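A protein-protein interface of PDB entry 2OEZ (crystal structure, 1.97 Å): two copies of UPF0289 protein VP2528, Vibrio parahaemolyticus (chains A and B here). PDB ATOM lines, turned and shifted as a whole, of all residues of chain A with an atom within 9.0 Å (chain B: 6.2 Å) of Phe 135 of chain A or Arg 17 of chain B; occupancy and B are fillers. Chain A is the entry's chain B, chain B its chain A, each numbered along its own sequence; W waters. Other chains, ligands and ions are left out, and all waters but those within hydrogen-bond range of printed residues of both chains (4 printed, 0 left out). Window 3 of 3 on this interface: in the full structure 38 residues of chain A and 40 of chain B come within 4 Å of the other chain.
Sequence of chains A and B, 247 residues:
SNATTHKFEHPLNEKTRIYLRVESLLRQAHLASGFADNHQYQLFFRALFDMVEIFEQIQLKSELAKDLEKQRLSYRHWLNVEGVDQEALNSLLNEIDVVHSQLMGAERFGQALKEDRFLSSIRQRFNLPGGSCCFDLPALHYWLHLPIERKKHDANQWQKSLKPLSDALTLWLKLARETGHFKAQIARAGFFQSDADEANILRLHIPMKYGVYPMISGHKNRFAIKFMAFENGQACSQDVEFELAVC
The backbone carbonyl oxygen (O) of Leu 20 of chain B is in hydrogen-bond range of the side-chain sulfur (SG) of Cys 133 of chain A.
NH2 of Arg 17 of chain B sits at hydrogen-bond distance from O of Pro 11 of chain B. The backbone carbonyl oxygen of Gly 131 of chain A is in hydrogen-bond range of the side-chain sulfur of Cys 133 of chain A, 3.6 Å away. The backbone carbonyl oxygen of Cys 133 of chain A sits close to the side-chain carboxylate of Asp 136 of chain A, 2.7 Å away.
Among the printed residues, merely in contact across the chains: Phe 135 of chain A with Glu 9 of chain B, Phe 135 of chain A with Arg 17 of chain B, Gly 131 of chain A with Arg 21 of chain B, Phe 135 of chain A with Leu 20 of chain B, Phe 135 of chain A with Pro 11 of chain B and Phe 135 of chain A with Arg 21 of chain B.
Of the printed residues of chain B, Phe 135 of chain A touches Glu 9, Pro 11, Arg 17, Leu 20 and Arg 21. Of the printed residues of chain A, Arg 17 of chain B touches Phe 135 (3.2 Å). No residue of chain A comes within 4 Å of Thr 16 of chain B. Printed residues of chain A within 4 Å of Leu 20 of chain B: Cys 133 (3.7 Å) and Phe 135 (3.4 Å). Of the printed residues of chain B, Gly 131 of chain A touches Arg 21 (3.2 Å). Of the printed residues of chain B, Cys 133 of chain A touches Leu 20. Printed residues of chain A within 4 Å of Arg 21 of chain B: Gly 131 (3.2 Å) and Phe 135 (3.5 Å). The nearest printed residue of chain A that does not touch Arg 17 of chain B is Asp 136 of chain A (5.5 Å). The nearest printed residue of chain A that does not touch Leu 20 of chain B is Gly 131 of chain A (5.0 Å).
Hydrophobic or aromatic side chains of chain A that line the printed part of chain B: Phe 135. Of the 15 printed residues of chain B, 5 touch a printed residue of chain A. Among the printed residues, 7 pairs touch across the chains. Among the printed residues, no Asp or Glu carboxylate lies within 4 Å of a Lys or Arg side-chain nitrogen of the other chain.
No position is printed for both chains.
Water W4 lies within hydrogen-bond range of the backbone carbonyl oxygen (O) of Phe 135 of chain A and a ring nitrogen (ND1) of His 10 of chain B. Water W2 bridges N of Gly 131 of chain A (2.7 Å) and NE of Arg 21 of chain B (2.8 Å). Water W3 bridges NH2 of Arg 21 of chain B (2.9 Å) and O of Pro 129 of chain A (3.0 Å). Water W1 bridges N of Glu 9 of chain B (3.1 Å) and NE2 of His 141 of chain A (3.3 Å).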
ATOM      1  N   TYR A  41     -41.991 -34.689  10.147  1.00  0.00           N
ATOM      2  CA  TYR A  41     -42.308 -33.937   8.920  1.00  0.00           C
ATOM      3  C   TYR A  41     -41.519 -34.574   7.789  1.00  0.00           C
ATOM      4  O   TYR A  41     -41.977 -34.608   6.672  1.00  0.00           O
ATOM      5  CB  TYR A  41     -41.925 -32.442   9.060  1.00  0.00           C
ATOM      6  CG  TYR A  41     -40.467 -32.199   8.921  1.00  0.00           C
ATOM      7  CD1 TYR A  41     -39.653 -32.135  10.036  1.00  0.00           C
ATOM      8  CD2 TYR A  41     -39.882 -32.064   7.669  1.00  0.00           C
ATOM      9  CE1 TYR A  41     -38.294 -31.902   9.919  1.00  0.00           C
ATOM     10  CE2 TYR A  41     -38.511 -31.845   7.536  1.00  0.00           C
ATOM     11  CZ  TYR A  41     -37.743 -31.767   8.657  1.00  0.00           C
ATOM     12  OH  TYR A  41     -36.406 -31.586   8.530  1.00  0.00           O
ATOM     13  N   ARG A 125     -36.207 -29.961  -4.808  1.00  0.00           N
ATOM     14  CA  ARG A 125     -35.154 -29.879  -3.826  1.00  0.00           C
ATOM     15  C   ARG A 125     -35.340 -30.914  -2.725  1.00  0.00           C
ATOM     16  O   ARG A 125     -34.378 -31.565  -2.314  1.00  0.00           O
ATOM     17  CB  ARG A 125     -35.064 -28.469  -3.268  1.00  0.00           C
ATOM     18  CG  ARG A 125     -34.230 -27.571  -4.171  1.00  0.00           C
ATOM     19  CD  ARG A 125     -34.885 -26.228  -4.418  1.00  0.00           C
ATOM     20  NE  ARG A 125     -34.607 -25.302  -3.333  1.00  0.00           N
ATOM     21  CZ  ARG A 125     -35.531 -24.611  -2.676  1.00  0.00           C
ATOM     22  NH1 ARG A 125     -36.834 -24.701  -2.994  1.00  0.00           N
ATOM     23  NH2 ARG A 125     -35.129 -23.800  -1.705  1.00  0.00           N
ATOM     24  N   PRO A 129     -30.863 -36.175  -2.155  1.00  0.00           N
ATOM     25  CA  PRO A 129     -30.219 -36.661  -0.894  1.00  0.00           C
ATOM     26  C   PRO A 129     -30.342 -35.669   0.273  1.00  0.00           C
ATOM     27  O   PRO A 129     -29.942 -34.496   0.135  1.00  0.00           O
ATOM     28  CB  PRO A 129     -28.750 -36.831  -1.283  1.00  0.00           C
ATOM     29  CG  PRO A 129     -28.642 -36.424  -2.765  1.00  0.00           C
ATOM     30  CD  PRO A 129     -30.017 -36.458  -3.333  1.00  0.00           C
ATOM     31  N   GLY A 130     -30.887 -36.133   1.405  1.00  0.00           N
ATOM     32  CA  GLY A 130     -31.520 -35.207   2.358  1.00  0.00           C
ATOM     33  C   GLY A 130     -31.402 -35.314   3.877  1.00  0.00           C
ATOM     34  O   GLY A 130     -32.258 -35.907   4.544  1.00  0.00           O
ATOM     35  N   GLY A 131     -30.378 -34.672   4.431  1.00  0.00           N
ATOM     36  CA  GLY A 131     -30.284 -34.515   5.873  1.00  0.00           C
ATOM     37  C   GLY A 131     -29.213 -33.529   6.267  1.00  0.00           C
ATOM     38  O   GLY A 131     -29.097 -32.480   5.654  1.00  0.00           O
ATOM     39  N   CYS A 133     -32.152 -31.982   7.174  1.00  0.00           N
ATOM     40  CA  CYS A 133     -32.407 -30.684   7.833  1.00  0.00           C
ATOM     41  C   CYS A 133     -32.877 -29.690   6.797  1.00  0.00           C
ATOM     42  O   CYS A 133     -33.225 -30.098   5.669  1.00  0.00           O
ATOM     43  CB  CYS A 133     -31.198 -30.144   8.628  1.00  0.00           C
ATOM     44  SG  CYS A 133     -29.683 -29.554   7.701  1.00  0.00           S
ATOM     45  N   CYS A 134     -32.898 -28.403   7.171  1.00  0.00           N
ATOM     46  CA  CYS A 134     -33.642 -27.394   6.410  1.00  0.00           C
ATOM     47  C   CYS A 134     -32.938 -26.078   6.122  1.00  0.00           C
ATOM     48  O   CYS A 134     -33.562 -25.168   5.584  1.00  0.00           O
ATOM     49  CB  CYS A 134     -34.996 -27.103   7.065  1.00  0.00           C
ATOM     50  SG  CYS A 134     -36.106 -28.494   6.997  1.00  0.00           S
ATOM     51  N   PHE A 135     -31.651 -25.969   6.441  1.00  0.00           N
ATOM     52  CA  PHE A 135     -30.898 -24.791   5.977  1.00  0.00           C
ATOM     53  C   PHE A 135     -30.960 -24.614   4.448  1.00  0.00           C
ATOM     54  O   PHE A 135     -30.770 -23.512   3.936  1.00  0.00           O
ATOM     55  CB  PHE A 135     -29.434 -24.788   6.498  1.00  0.00           C
ATOM     56  CG  PHE A 135     -28.590 -25.899   5.947  1.00  0.00           C
ATOM     57  CD1 PHE A 135     -28.085 -25.839   4.650  1.00  0.00           C
ATOM     58  CD2 PHE A 135     -28.312 -27.014   6.709  1.00  0.00           C
ATOM     59  CE1 PHE A 135     -27.311 -26.880   4.134  1.00  0.00           C
ATOM     60  CE2 PHE A 135     -27.538 -28.062   6.192  1.00  0.00           C
ATOM     61  CZ  PHE A 135     -27.033 -27.984   4.916  1.00  0.00           C
ATOM     62  N   ASP A 136     -31.224 -25.747   3.790  1.00  0.00           N
ATOM     63  CA  ASP A 136     -31.345 -25.891   2.352  1.00  0.00           C
ATOM     64  C   ASP A 136     -32.646 -25.326   1.834  1.00  0.00           C
ATOM     65  O   ASP A 136     -32.668 -24.713   0.764  1.00  0.00           O
ATOM     66  CB  ASP A 136     -31.232 -27.382   1.908  1.00  0.00           C
ATOM     67  CG  ASP A 136     -31.250 -28.392   3.080  1.00  0.00           C
ATOM     68  OD1 ASP A 136     -32.077 -28.263   4.002  1.00  0.00           O
ATOM     69  OD2 ASP A 136     -30.431 -29.345   3.058  1.00  0.00           O
ATOM     70  N   LEU A 137     -33.717 -25.560   2.599  1.00  0.00           N
ATOM     71  CA  LEU A 137     -35.101 -25.293   2.227  1.00  0.00           C
ATOM     72  C   LEU A 137     -35.731 -24.325   3.258  1.00  0.00           C
ATOM     73  O   LEU A 137     -36.603 -24.709   4.047  1.00  0.00           O
ATOM     74  CB  LEU A 137     -35.944 -26.591   2.200  1.00  0.00           C
ATOM     75  CG  LEU A 137     -35.933 -27.444   0.943  1.00  0.00           C
ATOM     76  CD1 LEU A 137     -36.449 -28.841   1.256  1.00  0.00           C
ATOM     77  CD2 LEU A 137     -36.782 -26.778  -0.065  1.00  0.00           C
ATOM     78  N   PRO A 138     -35.346 -23.054   3.213  1.00  0.00           N
ATOM     79  CA  PRO A 138     -35.924 -22.062   4.147  1.00  0.00           C
ATOM     80  C   PRO A 138     -37.456 -21.931   4.119  1.00  0.00           C
ATOM     81  O   PRO A 138     -38.026 -21.675   5.151  1.00  0.00           O
ATOM     82  CB  PRO A 138     -35.249 -20.728   3.748  1.00  0.00           C
ATOM     83  CG  PRO A 138     -34.565 -20.966   2.452  1.00  0.00           C
ATOM     84  CD  PRO A 138     -34.402 -22.481   2.242  1.00  0.00           C
ATOM     85  N   ALA A 139     -38.132 -22.106   2.996  1.00  0.00           N
ATOM     86  CA  ALA A 139     -39.598 -22.049   3.010  1.00  0.00           C
ATOM     87  C   ALA A 139     -40.196 -23.134   3.869  1.00  0.00           C
ATOM     88  O   ALA A 139     -41.229 -22.910   4.534  1.00  0.00           O
ATOM     89  CB  ALA A 139     -40.184 -22.158   1.637  1.00  0.00           C
ATOM     90  N   LEU A 140     -39.637 -24.345   3.759  1.00  0.00           N
ATOM     91  CA  LEU A 140     -40.041 -25.478   4.585  1.00  0.00           C
ATOM     92  C   LEU A 140     -39.724 -25.168   6.054  1.00  0.00           C
ATOM     93  O   LEU A 140     -40.557 -25.347   6.941  1.00  0.00           O
ATOM     94  CB  LEU A 140     -39.401 -26.805   4.103  1.00  0.00           C
ATOM     95  CG  LEU A 140     -39.617 -28.055   5.003  1.00  0.00           C
ATOM     96  CD1 LEU A 140     -41.099 -28.335   5.246  1.00  0.00           C
ATOM     97  CD2 LEU A 140     -38.952 -29.331   4.460  1.00  0.00           C
ATOM     98  N   HIS A 141     -38.527 -24.672   6.329  1.00  0.00           N
ATOM     99  CA  HIS A 141     -38.193 -24.371   7.682  1.00  0.00           C
ATOM    100  C   HIS A 141     -39.176 -23.344   8.314  1.00  0.00           C
ATOM    101  O   HIS A 141     -39.447 -23.411   9.506  1.00  0.00           O
ATOM    102  CB  HIS A 141     -36.775 -23.779   7.725  1.00  0.00           C
ATOM    103  CG  HIS A 141     -36.159 -23.752   9.092  1.00  0.00           C
ATOM    104  ND1 HIS A 141     -35.980 -22.592   9.817  1.00  0.00           N
ATOM    105  CD2 HIS A 141     -35.612 -24.749   9.833  1.00  0.00           C
ATOM    106  CE1 HIS A 141     -35.381 -22.882  10.960  1.00  0.00           C
ATOM    107  NE2 HIS A 141     -35.125 -24.181  10.981  1.00  0.00           N
ATOM    108  N   TYR A 142     -39.620 -22.341   7.533  1.00  0.00           N
ATOM    109  CA  TYR A 142     -40.560 -21.317   8.006  1.00  0.00           C
ATOM    110  C   TYR A 142     -41.865 -22.048   8.320  1.00  0.00           C
ATOM    111  O   TYR A 142     -42.544 -21.833   9.324  1.00  0.00           O
ATOM    112  CB  TYR A 142     -40.778 -20.304   6.848  1.00  0.00           C
ATOM    113  CG  TYR A 142     -41.911 -19.348   7.055  1.00  0.00           C
ATOM    114  CD1 TYR A 142     -41.674 -18.056   7.584  1.00  0.00           C
ATOM    115  CD2 TYR A 142     -43.237 -19.722   6.770  1.00  0.00           C
ATOM    116  CE1 TYR A 142     -42.713 -17.191   7.777  1.00  0.00           C
ATOM    117  CE2 TYR A 142     -44.278 -18.834   6.953  1.00  0.00           C
ATOM    118  CZ  TYR A 142     -44.002 -17.576   7.453  1.00  0.00           C
ATOM    119  OH  TYR A 142     -45.071 -16.695   7.674  1.00  0.00           O
ATOM    120  N   LEU A 144     -42.445 -25.059   9.218  1.00  0.00           N
ATOM    121  CA  LEU A 144     -42.350 -25.946  10.388  1.00  0.00           C
ATOM    122  C   LEU A 144     -42.503 -25.134  11.683  1.00  0.00           C
ATOM    123  O   LEU A 144     -42.856 -25.678  12.717  1.00  0.00           O
ATOM    124  CB  LEU A 144     -41.019 -26.711  10.374  1.00  0.00           C
ATOM    125  CG  LEU A 144     -40.988 -27.803   9.297  1.00  0.00           C
ATOM    126  CD1 LEU A 144     -39.593 -28.408   9.131  1.00  0.00           C
ATOM    127  CD2 LEU A 144     -42.031 -28.879   9.675  1.00  0.00           C
ATOM    128  N   GLU B   9     -30.505 -21.058  10.273  1.00  0.00           N
ATOM    129  CA  GLU B   9     -29.029 -21.150  10.147  1.00  0.00           C
ATOM    130  C   GLU B   9     -28.648 -21.387   8.706  1.00  0.00           C
ATOM    131  O   GLU B   9     -29.337 -22.123   7.993  1.00  0.00           O
ATOM    132  CB  GLU B   9     -28.460 -22.300  10.977  1.00  0.00           C
ATOM    133  CG  GLU B   9     -28.382 -21.958  12.385  1.00  0.00           C
ATOM    134  CD  GLU B   9     -27.583 -22.963  13.198  1.00  0.00           C
ATOM    135  OE1 GLU B   9     -27.530 -24.156  12.778  1.00  0.00           O
ATOM    136  OE2 GLU B   9     -27.026 -22.542  14.247  1.00  0.00           O
ATOM    137  N   HIS B  10     -27.559 -20.751   8.277  1.00  0.00           N
ATOM    138  CA  HIS B  10     -27.078 -20.846   6.898  1.00  0.00           C
ATOM    139  C   HIS B  10     -25.574 -21.148   6.930  1.00  0.00           C
ATOM    140  O   HIS B  10     -24.831 -20.378   7.488  1.00  0.00           O
ATOM    141  CB  HIS B  10     -27.324 -19.510   6.108  1.00  0.00           C
ATOM    142  CG  HIS B  10     -26.731 -19.526   4.721  1.00  0.00           C
ATOM    143  ND1 HIS B  10     -27.324 -20.187   3.671  1.00  0.00           N
ATOM    144  CD2 HIS B  10     -25.600 -18.978   4.223  1.00  0.00           C
ATOM    145  CE1 HIS B  10     -26.586 -20.046   2.580  1.00  0.00           C
ATOM    146  NE2 HIS B  10     -25.506 -19.347   2.900  1.00  0.00           N
ATOM    147  N   PRO B  11     -25.145 -22.256   6.303  1.00  0.00           N
ATOM    148  CA  PRO B  11     -23.719 -22.540   6.193  1.00  0.00           C
ATOM    149  C   PRO B  11     -23.134 -21.648   5.106  1.00  0.00           C
ATOM    150  O   PRO B  11     -23.746 -21.492   4.041  1.00  0.00           O
ATOM    151  CB  PRO B  11     -23.669 -23.995   5.732  1.00  0.00           C
ATOM    152  CG  PRO B  11     -25.003 -24.177   4.916  1.00  0.00           C
ATOM    153  CD  PRO B  11     -26.008 -23.252   5.617  1.00  0.00           C
ATOM    154  N   LEU B  12     -21.944 -21.120   5.347  1.00  0.00           N
ATOM    155  CA  LEU B  12     -21.376 -20.196   4.411  1.00  0.00           C
ATOM    156  C   LEU B  12     -20.370 -20.857   3.504  1.00  0.00           C
ATOM    157  O   LEU B  12     -19.804 -20.164   2.664  1.00  0.00           O
ATOM    158  CB  LEU B  12     -20.702 -19.018   5.126  1.00  0.00           C
ATOM    159  CG  LEU B  12     -21.660 -18.044   5.837  1.00  0.00           C
ATOM    160  CD1 LEU B  12     -20.963 -17.246   6.949  1.00  0.00           C
ATOM    161  CD2 LEU B  12     -22.185 -17.078   4.719  1.00  0.00           C
ATOM    162  N   ASN B  13     -20.090 -22.146   3.689  1.00  0.00           N
ATOM    163  CA  ASN B  13     -19.113 -22.830   2.807  1.00  0.00           C
ATOM    164  C   ASN B  13     -19.499 -24.295   2.734  1.00  0.00           C
ATOM    165  O   ASN B  13     -20.372 -24.755   3.518  1.00  0.00           O
ATOM    166  CB  ASN B  13     -17.676 -22.599   3.300  1.00  0.00           C
ATOM    167  CG  ASN B  13     -17.520 -22.877   4.793  1.00  0.00           C
ATOM    168  OD1 ASN B  13     -17.812 -23.987   5.267  1.00  0.00           O
ATOM    169  ND2 ASN B  13     -17.112 -21.862   5.542  1.00  0.00           N
ATOM    170  N   GLU B  14     -18.927 -25.031   1.785  1.00  0.00           N
ATOM    171  CA  GLU B  14     -19.331 -26.417   1.585  1.00  0.00           C
ATOM    172  C   GLU B  14     -19.040 -27.326   2.798  1.00  0.00           C
ATOM    173  O   GLU B  14     -19.812 -28.239   3.064  1.00  0.00           O
ATOM    174  CB  GLU B  14     -18.724 -27.013   0.288  1.00  0.00           C
ATOM    175  CG  GLU B  14     -19.011 -26.188  -0.987  1.00  0.00           C
ATOM    176  CD  GLU B  14     -20.311 -26.562  -1.716  1.00  0.00           C
ATOM    177  OE1 GLU B  14     -21.375 -26.735  -1.067  1.00  0.00           O
ATOM    178  OE2 GLU B  14     -20.248 -26.668  -2.971  1.00  0.00           O
ATOM    179  N   LYS B  15     -17.945 -27.087   3.526  1.00  0.00           N
ATOM    180  CA  LYS B  15     -17.600 -27.953   4.657  1.00  0.00           C
ATOM    181  C   LYS B  15     -18.609 -27.794   5.806  1.00  0.00           C
ATOM    182  O   LYS B  15     -19.033 -28.763   6.425  1.00  0.00           O
ATOM    183  CB  LYS B  15     -16.194 -27.605   5.147  1.00  0.00           C
ATOM    184  CG  LYS B  15     -15.919 -27.951   6.596  1.00  0.00           C
ATOM    185  CD  LYS B  15     -14.886 -26.975   7.182  1.00  0.00           C
ATOM    186  CE  LYS B  15     -15.513 -25.735   7.837  1.00  0.00           C
ATOM    187  NZ  LYS B  15     -14.502 -25.111   8.762  1.00  0.00           N
ATOM    188  N   THR B  16     -19.059 -26.556   6.035  1.00  0.00           N
ATOM    189  CA  THR B  16     -20.034 -26.311   7.051  1.00  0.00           C
ATOM    190  C   THR B  16     -21.414 -26.858   6.647  1.00  0.00           C
ATOM    191  O   THR B  16     -22.197 -27.278   7.486  1.00  0.00           O
ATOM    192  CB  THR B  16     -20.162 -24.802   7.384  1.00  0.00           C
ATOM    193  OG1 THR B  16     -18.867 -24.294   7.766  1.00  0.00           O
ATOM    194  CG2 THR B  16     -21.117 -24.638   8.574  1.00  0.00           C
ATOM    195  N   ARG B  17     -21.721 -26.836   5.349  1.00  0.00           N
ATOM    196  CA  ARG B  17     -22.972 -27.411   4.827  1.00  0.00           C
ATOM    197  C   ARG B  17     -22.988 -28.959   5.111  1.00  0.00           C
ATOM    198  O   ARG B  17     -24.029 -29.538   5.400  1.00  0.00           O
ATOM    199  CB  ARG B  17     -23.091 -27.061   3.320  1.00  0.00           C
ATOM    200  CG  ARG B  17     -24.499 -27.191   2.656  1.00  0.00           C
ATOM    201  CD  ARG B  17     -24.755 -26.260   1.353  1.00  0.00           C
ATOM    202  NE  ARG B  17     -24.262 -24.853   1.393  1.00  0.00           N
ATOM    203  CZ  ARG B  17     -25.007 -23.740   1.499  1.00  0.00           C
ATOM    204  NH1 ARG B  17     -26.329 -23.812   1.608  1.00  0.00           N
ATOM    205  NH2 ARG B  17     -24.408 -22.529   1.515  1.00  0.00           N
ATOM    206  N   ILE B  18     -21.831 -29.611   5.037  1.00  0.00           N
ATOM    207  CA  ILE B  18     -21.713 -31.034   5.441  1.00  0.00           C
ATOM    208  C   ILE B  18     -21.881 -31.216   6.963  1.00  0.00           C
ATOM    209  O   ILE B  18     -22.536 -32.113   7.403  1.00  0.00           O
ATOM    210  CB  ILE B  18     -20.326 -31.564   5.052  1.00  0.00           C
ATOM    211  CG1 ILE B  18     -20.131 -31.543   3.520  1.00  0.00           C
ATOM    212  CG2 ILE B  18     -20.077 -32.993   5.681  1.00  0.00           C
ATOM    213  CD1 ILE B  18     -21.231 -32.264   2.817  1.00  0.00           C
ATOM    214  N   TYR B  19     -21.230 -30.372   7.759  1.00  0.00           N
ATOM    215  CA  TYR B  19     -21.362 -30.387   9.225  1.00  0.00           C
ATOM    216  C   TYR B  19     -22.807 -30.303   9.629  1.00  0.00           C
ATOM    217  O   TYR B  19     -23.233 -31.067  10.462  1.00  0.00           O
ATOM    218  CB  TYR B  19     -20.641 -29.193   9.863  1.00  0.00           C
ATOM    219  CG  TYR B  19     -19.136 -29.277   9.869  1.00  0.00           C
ATOM    220  CD1 TYR B  19     -18.462 -30.392   9.375  1.00  0.00           C
ATOM    221  CD2 TYR B  19     -18.387 -28.236  10.405  1.00  0.00           C
ATOM    222  CE1 TYR B  19     -17.061 -30.451   9.394  1.00  0.00           C
ATOM    223  CE2 TYR B  19     -17.005 -28.296  10.441  1.00  0.00           C
ATOM    224  CZ  TYR B  19     -16.360 -29.421   9.947  1.00  0.00           C
ATOM    225  OH  TYR B  19     -14.994 -29.479   9.992  1.00  0.00           O
ATOM    226  N   LEU B  20     -23.534 -29.315   9.097  1.00  0.00           N
ATOM    227  CA  LEU B  20     -24.922 -29.142   9.475  1.00  0.00           C
ATOM    228  C   LEU B  20     -25.765 -30.322   9.010  1.00  0.00           C
ATOM    229  O   LEU B  20     -26.724 -30.678   9.674  1.00  0.00           O
ATOM    230  CB  LEU B  20     -25.552 -27.837   8.938  1.00  0.00           C
ATOM    231  CG  LEU B  20     -24.901 -26.549   9.548  1.00  0.00           C
ATOM    232  CD1 LEU B  20     -25.625 -25.290   8.994  1.00  0.00           C
ATOM    233  CD2 LEU B  20     -24.957 -26.593  11.091  1.00  0.00           C
ATOM    234  N   ARG B  21     -25.492 -30.834   7.819  1.00  0.00           N
ATOM    235  CA  ARG B  21     -26.242 -31.988   7.312  1.00  0.00           C
ATOM    236  C   ARG B  21     -25.994 -33.240   8.205  1.00  0.00           C
ATOM    237  O   ARG B  21     -26.901 -33.981   8.498  1.00  0.00           O
ATOM    238  CB  ARG B  21     -25.823 -32.373   5.882  1.00  0.00           C
ATOM    239  CG  ARG B  21     -26.226 -31.388   4.752  1.00  0.00           C
ATOM    240  CD  ARG B  21     -25.552 -31.739   3.366  1.00  0.00           C
ATOM    241  NE  ARG B  21     -25.859 -33.086   2.902  1.00  0.00           N
ATOM    242  CZ  ARG B  21     -25.142 -33.773   1.995  1.00  0.00           C
ATOM    243  NH1 ARG B  21     -24.049 -33.250   1.445  1.00  0.00           N
ATOM    244  NH2 ARG B  21     -25.502 -35.014   1.654  1.00  0.00           N
ATOM    245  N   VAL B  22     -24.759 -33.440   8.635  1.00  0.00           N
ATOM    246  CA  VAL B  22     -24.400 -34.616   9.449  1.00  0.00           C
ATOM    247  C   VAL B  22     -25.033 -34.450  10.810  1.00  0.00           C
ATOM    248  O   VAL B  22     -25.526 -35.411  11.344  1.00  0.00           O
ATOM    249  CB  VAL B  22     -22.838 -34.846   9.494  1.00  0.00           C
ATOM    250  CG1 VAL B  22     -22.414 -35.986  10.497  1.00  0.00           C
ATOM    251  CG2 VAL B  22     -22.318 -35.225   8.084  1.00  0.00           C
ATOM    252  N   ILE B 216     -30.525 -16.865   1.080  1.00  0.00           N
ATOM    253  CA  ILE B 216     -29.209 -16.345   1.368  1.00  0.00           C
ATOM    254  C   ILE B 216     -28.223 -16.865   0.358  1.00  0.00           C
ATOM    255  O   ILE B 216     -28.212 -18.047   0.093  1.00  0.00           O
ATOM    256  CB  ILE B 216     -28.748 -16.759   2.765  1.00  0.00           C
ATOM    257  CG1 ILE B 216     -29.760 -16.224   3.826  1.00  0.00           C
ATOM    258  CG2 ILE B 216     -27.320 -16.213   3.055  1.00  0.00           C
ATOM    259  CD1 ILE B 216     -29.541 -16.782   5.213  1.00  0.00           C
HETATM  260  O   HOH W   1     -32.247 -23.485   9.541  1.00  0.00           O
HETATM  261  O   HOH W   2     -27.871 -34.961   3.424  1.00  0.00           O
HETATM  262  O   HOH W   3     -27.164 -33.414  -0.031  1.00  0.00           O
HETATM  263  O   HOH W   4     -30.057 -21.023   3.379  1.00  0.00           O
